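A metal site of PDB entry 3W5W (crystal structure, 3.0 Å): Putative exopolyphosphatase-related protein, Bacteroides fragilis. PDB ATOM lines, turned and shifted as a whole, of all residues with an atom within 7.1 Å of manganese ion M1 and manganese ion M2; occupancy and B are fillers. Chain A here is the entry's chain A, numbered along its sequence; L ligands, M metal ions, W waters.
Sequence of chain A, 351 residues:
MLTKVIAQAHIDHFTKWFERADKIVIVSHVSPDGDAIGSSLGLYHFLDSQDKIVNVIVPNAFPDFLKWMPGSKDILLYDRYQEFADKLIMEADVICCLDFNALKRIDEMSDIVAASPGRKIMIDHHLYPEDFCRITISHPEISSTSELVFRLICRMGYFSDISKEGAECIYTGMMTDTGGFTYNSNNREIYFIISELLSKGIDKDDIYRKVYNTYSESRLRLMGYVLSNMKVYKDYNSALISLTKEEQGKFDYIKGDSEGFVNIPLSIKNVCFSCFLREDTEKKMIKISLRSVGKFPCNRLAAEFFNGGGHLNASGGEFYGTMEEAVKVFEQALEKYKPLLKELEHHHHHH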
ATOM      1  N   SER A  28      13.050   6.400  13.540  1.00  0.00           N
ATOM      2  CA  SER A  28      11.622   6.678  13.690  1.00  0.00           C
ATOM      3  C   SER A  28      10.831   5.373  13.474  1.00  0.00           C
ATOM      4  O   SER A  28      11.410   4.371  13.093  1.00  0.00           O
ATOM      5  CB  SER A  28      11.161   7.762  12.722  1.00  0.00           C
ATOM      6  OG  SER A  28       9.872   8.233  13.064  1.00  0.00           O
ATOM      7  N   HIS A  29       9.512   5.405  13.695  1.00  0.00           N
ATOM      8  CA  HIS A  29       8.674   4.205  13.608  1.00  0.00           C
ATOM      9  C   HIS A  29       8.372   3.597  12.239  1.00  0.00           C
ATOM     10  O   HIS A  29       8.411   4.280  11.220  1.00  0.00           O
ATOM     11  CB  HIS A  29       7.353   4.455  14.333  1.00  0.00           C
ATOM     12  CG  HIS A  29       6.496   5.489  13.674  1.00  0.00           C
ATOM     13  ND1 HIS A  29       5.740   5.221  12.551  1.00  0.00           N
ATOM     14  CD2 HIS A  29       6.281   6.788  13.969  1.00  0.00           C
ATOM     15  CE1 HIS A  29       5.085   6.309  12.191  1.00  0.00           C
ATOM     16  NE2 HIS A  29       5.401   7.287  13.028  1.00  0.00           N
ATOM     17  N   SER A  31       6.639   2.360   8.941  1.00  0.00           N
ATOM     18  CA  SER A  31       5.644   3.113   8.184  1.00  0.00           C
ATOM     19  C   SER A  31       5.717   4.573   8.617  1.00  0.00           C
ATOM     20  O   SER A  31       4.786   5.126   9.210  1.00  0.00           O
ATOM     21  CB  SER A  31       4.232   2.583   8.445  1.00  0.00           C
ATOM     22  OG  SER A  31       4.065   1.319   7.836  1.00  0.00           O
ATOM     23  N   PRO A  32       6.846   5.225   8.345  1.00  0.00           N
ATOM     24  CA  PRO A  32       7.002   6.627   8.722  1.00  0.00           C
ATOM     25  C   PRO A  32       5.942   7.488   8.057  1.00  0.00           C
ATOM     26  O   PRO A  32       5.648   7.331   6.861  1.00  0.00           O
ATOM     27  CB  PRO A  32       8.408   6.965   8.226  1.00  0.00           C
ATOM     28  CG  PRO A  32       9.099   5.648   8.215  1.00  0.00           C
ATOM     29  CD  PRO A  32       8.054   4.737   7.661  1.00  0.00           C
ATOM     30  N   ASP A  33       5.368   8.396   8.833  1.00  0.00           N
ATOM     31  CA  ASP A  33       4.363   9.309   8.325  1.00  0.00           C
ATOM     32  C   ASP A  33       4.981  10.700   8.366  1.00  0.00           C
ATOM     33  O   ASP A  33       6.123  10.867   8.800  1.00  0.00           O
ATOM     34  CB  ASP A  33       3.142   9.274   9.236  1.00  0.00           C
ATOM     35  CG  ASP A  33       3.459   9.663  10.658  1.00  0.00           C
ATOM     36  OD1 ASP A  33       4.081   8.871  11.377  1.00  0.00           O
ATOM     37  OD2 ASP A  33       3.103  10.801  11.053  1.00  0.00           O
ATOM     38  N   GLY A  34       4.226  11.690   7.905  1.00  0.00           N
ATOM     39  CA  GLY A  34       4.705  13.066   7.889  1.00  0.00           C
ATOM     40  C   GLY A  34       5.466  13.548   9.121  1.00  0.00           C
ATOM     41  O   GLY A  34       6.511  14.192   8.999  1.00  0.00           O
ATOM     42  N   ASP A  35       4.963  13.238  10.313  1.00  0.00           N
ATOM     43  CA  ASP A  35       5.642  13.681  11.527  1.00  0.00           C
ATOM     44  C   ASP A  35       6.948  12.929  11.676  1.00  0.00           C
ATOM     45  O   ASP A  35       7.975  13.516  12.027  1.00  0.00           O
ATOM     46  CB  ASP A  35       4.751  13.463  12.754  1.00  0.00           C
ATOM     47  CG  ASP A  35       5.249  14.207  13.995  1.00  0.00           C
ATOM     48  OD1 ASP A  35       5.915  15.254  13.851  1.00  0.00           O
ATOM     49  OD2 ASP A  35       4.966  13.744  15.126  1.00  0.00           O
ATOM     50  N   ALA A  36       6.929  11.628  11.396  1.00  0.00           N
ATOM     51  CA  ALA A  36       8.133  10.812  11.519  1.00  0.00           C
ATOM     52  C   ALA A  36       9.273  11.344  10.643  1.00  0.00           C
ATOM     53  O   ALA A  36      10.355  11.635  11.143  1.00  0.00           O
ATOM     54  CB  ALA A  36       7.805   9.372  11.157  1.00  0.00           C
ATOM     55  N   ILE A  37       9.025  11.465   9.356  1.00  0.00           N
ATOM     56  CA  ILE A  37      10.037  11.969   8.422  1.00  0.00           C
ATOM     57  C   ILE A  37      10.402  13.444   8.657  1.00  0.00           C
ATOM     58  O   ILE A  37      11.569  13.825   8.575  1.00  0.00           O
ATOM     59  CB  ILE A  37       9.561  11.812   6.948  1.00  0.00           C
ATOM     60  CG1 ILE A  37       9.381  10.328   6.622  1.00  0.00           C
ATOM     61  CG2 ILE A  37      10.560  12.493   5.996  1.00  0.00           C
ATOM     62  CD1 ILE A  37      10.558   9.460   7.007  1.00  0.00           C
ATOM     63  N   SER A  39      10.087  15.415  11.534  1.00  0.00           N
ATOM     64  CA  SER A  39      10.806  15.648  12.783  1.00  0.00           C
ATOM     65  C   SER A  39      12.235  15.129  12.701  1.00  0.00           C
ATOM     66  O   SER A  39      13.152  15.711  13.295  1.00  0.00           O
ATOM     67  CB  SER A  39      10.105  14.950  13.934  1.00  0.00           C
ATOM     68  OG  SER A  39      10.199  13.548  13.775  1.00  0.00           O
ATOM     69  N   LEU A  98      12.737   9.306  17.580  1.00  0.00           N
ATOM     70  CA  LEU A  98      11.686  10.286  17.419  1.00  0.00           C
ATOM     71  C   LEU A  98      10.347   9.744  16.976  1.00  0.00           C
ATOM     72  O   LEU A  98      10.260   8.907  16.082  1.00  0.00           O
ATOM     73  CB  LEU A  98      12.131  11.372  16.439  1.00  0.00           C
ATOM     74  CG  LEU A  98      13.028  12.476  17.000  1.00  0.00           C
ATOM     75  CD1 LEU A  98      14.338  11.911  17.523  1.00  0.00           C
ATOM     76  CD2 LEU A  98      13.293  13.487  15.901  1.00  0.00           C
ATOM     77  N   ASP A  99       9.295  10.211  17.644  1.00  0.00           N
ATOM     78  CA  ASP A  99       7.945   9.842  17.278  1.00  0.00           C
ATOM     79  C   ASP A  99       7.460   8.405  17.534  1.00  0.00           C
ATOM     80  O   ASP A  99       6.591   7.899  16.810  1.00  0.00           O
ATOM     81  CB  ASP A  99       7.738  10.232  15.818  1.00  0.00           C
ATOM     82  CG  ASP A  99       6.304  10.498  15.496  1.00  0.00           C
ATOM     83  OD1 ASP A  99       5.690  11.318  16.195  1.00  0.00           O
ATOM     84  OD2 ASP A  99       5.809   9.881  14.533  1.00  0.00           O
ATOM     85  N   PHE A 100       8.000   7.764  18.557  1.00  0.00           N
ATOM     86  CA  PHE A 100       7.560   6.426  18.959  1.00  0.00           C
ATOM     87  C   PHE A 100       8.092   6.238  20.365  1.00  0.00           C
ATOM     88  O   PHE A 100       9.109   6.823  20.736  1.00  0.00           O
ATOM     89  CB  PHE A 100       8.098   5.336  18.019  1.00  0.00           C
ATOM     90  CG  PHE A 100       9.560   5.056  18.172  1.00  0.00           C
ATOM     91  CD1 PHE A 100      10.511   5.812  17.502  1.00  0.00           C
ATOM     92  CD2 PHE A 100      10.001   3.998  18.976  1.00  0.00           C
ATOM     93  CE1 PHE A 100      11.873   5.534  17.616  1.00  0.00           C
ATOM     94  CE2 PHE A 100      11.366   3.706  19.094  1.00  0.00           C
ATOM     95  CZ  PHE A 100      12.300   4.479  18.419  1.00  0.00           C
ATOM     96  N   ARG A 105       7.654  -0.560  18.093  1.00  0.00           N
ATOM     97  CA  ARG A 105       7.269   0.378  17.048  1.00  0.00           C
ATOM     98  C   ARG A 105       8.231   0.457  15.877  1.00  0.00           C
ATOM     99  O   ARG A 105       7.822   0.755  14.752  1.00  0.00           O
ATOM    100  CB  ARG A 105       7.082   1.769  17.654  1.00  0.00           C
ATOM    101  CG  ARG A 105       5.849   1.884  18.533  1.00  0.00           C
ATOM    102  CD  ARG A 105       4.624   1.649  17.708  1.00  0.00           C
ATOM    103  NE  ARG A 105       4.502   2.676  16.693  1.00  0.00           N
ATOM    104  CZ  ARG A 105       3.829   2.507  15.559  1.00  0.00           C
ATOM    105  NH1 ARG A 105       3.238   1.354  15.315  1.00  0.00           N
ATOM    106  NH2 ARG A 105       3.763   3.498  14.674  1.00  0.00           N
ATOM    107  N   ASP A 124       9.015  12.115  21.956  1.00  0.00           N
ATOM    108  CA  ASP A 124       7.735  11.622  21.473  1.00  0.00           C
ATOM    109  C   ASP A 124       6.533  12.326  22.100  1.00  0.00           C
ATOM    110  O   ASP A 124       6.670  13.082  23.054  1.00  0.00           O
ATOM    111  CB  ASP A 124       7.640  10.123  21.775  1.00  0.00           C
ATOM    112  CG  ASP A 124       6.372   9.497  21.262  1.00  0.00           C
ATOM    113  OD1 ASP A 124       6.135   9.589  20.036  1.00  0.00           O
ATOM    114  OD2 ASP A 124       5.619   8.922  22.071  1.00  0.00           O
ATOM    115  N   HIS A 125       5.340  12.050  21.561  1.00  0.00           N
ATOM    116  CA  HIS A 125       4.115  12.638  22.084  1.00  0.00           C
ATOM    117  C   HIS A 125       2.968  11.633  22.140  1.00  0.00           C
ATOM    118  O   HIS A 125       1.799  12.011  22.159  1.00  0.00           O
ATOM    119  CB  HIS A 125       3.670  13.845  21.243  1.00  0.00           C
ATOM    120  CG  HIS A 125       3.274  13.498  19.851  1.00  0.00           C
ATOM    121  ND1 HIS A 125       2.142  14.000  19.246  1.00  0.00           N
ATOM    122  CD2 HIS A 125       3.875  12.720  18.918  1.00  0.00           C
ATOM    123  CE1 HIS A 125       2.063  13.557  18.014  1.00  0.00           C
ATOM    124  NE2 HIS A 125       3.107  12.778  17.776  1.00  0.00           N
ATOM    125  N   HIS A 126       3.302  10.351  22.154  1.00  0.00           N
ATOM    126  CA  HIS A 126       2.278   9.322  22.232  1.00  0.00           C
ATOM    127  C   HIS A 126       2.119   8.929  23.708  1.00  0.00           C
ATOM    128  O   HIS A 126       3.017   9.165  24.503  1.00  0.00           O
ATOM    129  CB  HIS A 126       2.713   8.129  21.373  1.00  0.00           C
ATOM    130  CG  HIS A 126       2.683   8.436  19.907  1.00  0.00           C
ATOM    131  ND1 HIS A 126       1.555   8.281  19.134  1.00  0.00           N
ATOM    132  CD2 HIS A 126       3.632   8.947  19.084  1.00  0.00           C
ATOM    133  CE1 HIS A 126       1.802   8.695  17.900  1.00  0.00           C
ATOM    134  NE2 HIS A 126       3.060   9.100  17.848  1.00  0.00           N
ATOM    135  N   SER A 143       0.928  18.305  20.104  1.00  0.00           N
ATOM    136  CA  SER A 143       0.416  17.760  18.843  1.00  0.00           C
ATOM    137  C   SER A 143       1.333  17.011  17.880  1.00  0.00           C
ATOM    138  O   SER A 143       0.827  16.287  17.016  1.00  0.00           O
ATOM    139  CB  SER A 143      -0.305  18.868  18.063  1.00  0.00           C
ATOM    140  OG  SER A 143       0.567  19.953  17.790  1.00  0.00           O
ATOM    141  N   SER A 144       2.644  17.167  18.002  1.00  0.00           N
ATOM    142  CA  SER A 144       3.565  16.477  17.091  1.00  0.00           C
ATOM    143  C   SER A 144       4.968  16.315  17.653  1.00  0.00           C
ATOM    144  O   SER A 144       5.352  17.026  18.559  1.00  0.00           O
ATOM    145  CB  SER A 144       3.663  17.268  15.768  1.00  0.00           C
ATOM    146  OG  SER A 144       4.189  18.562  15.980  1.00  0.00           O
ATOM    147  N   THR A 145       5.725  15.370  17.094  1.00  0.00           N
ATOM    148  CA  THR A 145       7.098  15.181  17.545  1.00  0.00           C
ATOM    149  C   THR A 145       7.863  16.340  16.926  1.00  0.00           C
ATOM    150  O   THR A 145       8.731  16.941  17.570  1.00  0.00           O
ATOM    151  CB  THR A 145       7.689  13.821  17.059  1.00  0.00           C
ATOM    152  OG1 THR A 145       7.070  12.741  17.771  1.00  0.00           O
ATOM    153  CG2 THR A 145       9.186  13.767  17.328  1.00  0.00           C
ATOM    154  N   SER A 146       7.513  16.674  15.685  1.00  0.00           N
ATOM    155  CA  SER A 146       8.135  17.795  14.975  1.00  0.00           C
ATOM    156  C   SER A 146       8.188  19.067  15.822  1.00  0.00           C
ATOM    157  O   SER A 146       9.185  19.780  15.841  1.00  0.00           O
ATOM    158  CB  SER A 146       7.374  18.113  13.683  1.00  0.00           C
ATOM    159  OG  SER A 146       7.320  17.007  12.817  1.00  0.00           O
ATOM    160  N   GLY A 173       5.900  18.060   9.524  1.00  0.00           N
ATOM    161  CA  GLY A 173       5.557  17.139  10.591  1.00  0.00           C
ATOM    162  C   GLY A 173       4.392  17.661  11.434  1.00  0.00           C
ATOM    163  O   GLY A 173       3.506  16.892  11.809  1.00  0.00           O
ATOM    164  N   THR A 176       1.067  17.594   9.237  1.00  0.00           N
ATOM    165  CA  THR A 176       0.633  16.222   9.120  1.00  0.00           C
ATOM    166  C   THR A 176      -0.088  15.659  10.337  1.00  0.00           C
ATOM    167  O   THR A 176      -1.166  15.091  10.203  1.00  0.00           O
ATOM    168  CB  THR A 176       1.831  15.317   8.818  1.00  0.00           C
ATOM    169  OG1 THR A 176       1.957  15.181   7.405  1.00  0.00           O
ATOM    170  CG2 THR A 176       1.668  13.918   9.486  1.00  0.00           C
ATOM    171  N   ASP A 177       0.508  15.794  11.505  1.00  0.00           N
ATOM    172  CA  ASP A 177      -0.097  15.258  12.720  1.00  0.00           C
ATOM    173  C   ASP A 177      -1.323  15.979  13.223  1.00  0.00           C
ATOM    174  O   ASP A 177      -1.917  15.583  14.216  1.00  0.00           O
ATOM    175  CB  ASP A 177       0.951  15.166  13.820  1.00  0.00           C
ATOM    176  CG  ASP A 177       1.510  13.765  13.964  1.00  0.00           C
ATOM    177  OD1 ASP A 177       1.473  12.994  12.975  1.00  0.00           O
ATOM    178  OD2 ASP A 177       1.995  13.445  15.071  1.00  0.00           O
ATOM    179  N   HIS A 311      -4.191   4.181  18.405  1.00  0.00           N
ATOM    180  CA  HIS A 311      -4.538   5.311  19.260  1.00  0.00           C
ATOM    181  C   HIS A 311      -6.039   5.528  19.386  1.00  0.00           C
ATOM    182  O   HIS A 311      -6.834   4.913  18.689  1.00  0.00           O
ATOM    183  CB  HIS A 311      -3.861   6.576  18.722  1.00  0.00           C
ATOM    184  CG  HIS A 311      -2.408   6.393  18.430  1.00  0.00           C
ATOM    185  ND1 HIS A 311      -1.514   5.916  19.356  1.00  0.00           N
ATOM    186  CD2 HIS A 311      -1.700   6.569  17.281  1.00  0.00           C
ATOM    187  CE1 HIS A 311      -0.322   5.801  18.801  1.00  0.00           C
ATOM    188  NE2 HIS A 311      -0.408   6.193  17.546  1.00  0.00           N
HETATM  189  P1  LIG L   1      -4.126   3.011   9.797  1.00  0.00           P
HETATM  190  O1  LIG L   1      -3.377   3.969   8.946  1.00  0.00           O
HETATM  191  O2  LIG L   1      -3.690   1.499   9.425  1.00  0.00           O
HETATM  192  O3  LIG L   1      -5.705   3.178   9.537  1.00  0.00           O
HETATM  193  O4  LIG L   1      -3.817   3.311  11.365  1.00  0.00           O
HETATM  194  C1  LIG L   1      -2.408   3.154  11.578  1.00  0.00           C
HETATM  195  C2  LIG L   1      -2.062   3.406  13.052  1.00  0.00           C
HETATM  196  O5  LIG L   1      -2.783   2.479  13.920  1.00  0.00           O
HETATM  197  C3  LIG L   1      -0.551   3.228  13.294  1.00  0.00           C
HETATM  198  O6  LIG L   1       0.033   4.421  13.839  1.00  0.00           O
HETATM  199  C4  LIG L   1      -0.404   2.020  14.247  1.00  0.00           C
HETATM  200  O7  LIG L   1       0.284   2.381  15.442  1.00  0.00           O
HETATM  201  C5  LIG L   1      -1.843   1.532  14.537  1.00  0.00           C
HETATM  202  N1  LIG L   1      -2.071   0.139  14.029  1.00  0.00           N
HETATM  203  C6  LIG L   1      -2.551  -0.216  12.786  1.00  0.00           C
HETATM  204  N2  LIG L   1      -2.631  -1.517  12.683  1.00  0.00           N
HETATM  205  C7  LIG L   1      -2.210  -2.080  13.841  1.00  0.00           C
HETATM  206  C8  LIG L   1      -2.079  -3.430  14.299  1.00  0.00           C
HETATM  207  O8  LIG L   1      -2.385  -4.368  13.583  1.00  0.00           O
HETATM  208  N3  LIG L   1      -1.608  -3.654  15.573  1.00  0.00           N
HETATM  209  C9  LIG L   1      -1.263  -2.594  16.396  1.00  0.00           C
HETATM  210  N4  LIG L   1      -0.799  -2.846  17.662  1.00  0.00           N
HETATM  211  N5  LIG L   1      -1.389  -1.330  15.977  1.00  0.00           N
HETATM  212  C10 LIG L   1      -1.842  -1.031  14.723  1.00  0.00           C
HETATM  213 MN    MN M   1       3.850   9.339  13.558  1.00  0.00          MN
HETATM  214 MN    MN M   2       3.666  12.094  15.677  1.00  0.00          MN
HETATM  215  O   HOH W   1       1.056  10.345  15.037  1.00  0.00           O
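OD2 of Asp 124 lies within hydrogen-bond range of N of His 126 (2.7 Å).
The backbone NH (N) of Asp 99 sits close to the side-chain hydroxyl (OG1) of Thr 145 (3.4 Å).
A ring nitrogen (NE2) of His 311 sits close to a ring nitrogen (ND1) of His 126, 3.3 Å away.
OD1 of Asp 35 is in hydrogen-bond range of OG of Ser 146, at 2.5 Å.
OD1 of Asp 35 lies within hydrogen-bond range of N of Thr 145.
ND1 of His 29 sits close to O of Ser 31 (3.5 Å).
The backbone NH (N) of Ser 144 is in hydrogen-bond range of a ring nitrogen (ND1) of His 125.
The backbone carbonyl oxygen of Ser 143 sits close to a ring nitrogen (ND1) of His 125.
Manganese ion M1 is bound by the side-chain carboxylate of Asp 33, the side-chain carboxylate of Asp 99 and a ring nitrogen (NE2) of His 29.
Merely in contact with manganese ion M2: His 126.
Of the 25 residues printed, 5 come within 4 Å of manganese ion M2.
An oxygen (O7) of the ligand sits at hydrogen-bond distance from the guanidinium group (NH1) of Arg 105, 3.1 Å away.
Of the 25 residues printed, 3 come within 4 Å of manganese ion M1.
OD2 of Asp 35 is bound to manganese ion M2, 2.2 Å away.
The side-chain carboxylate (OD1) of Asp 99 binds manganese ion M2, at 2.2 Å.
The side-chain carboxylate (OD2) of Asp 177 is bound to manganese ion M2, at 2.2 Å.
NE2 of His 125 is bound to manganese ion M2 (2.3 Å).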
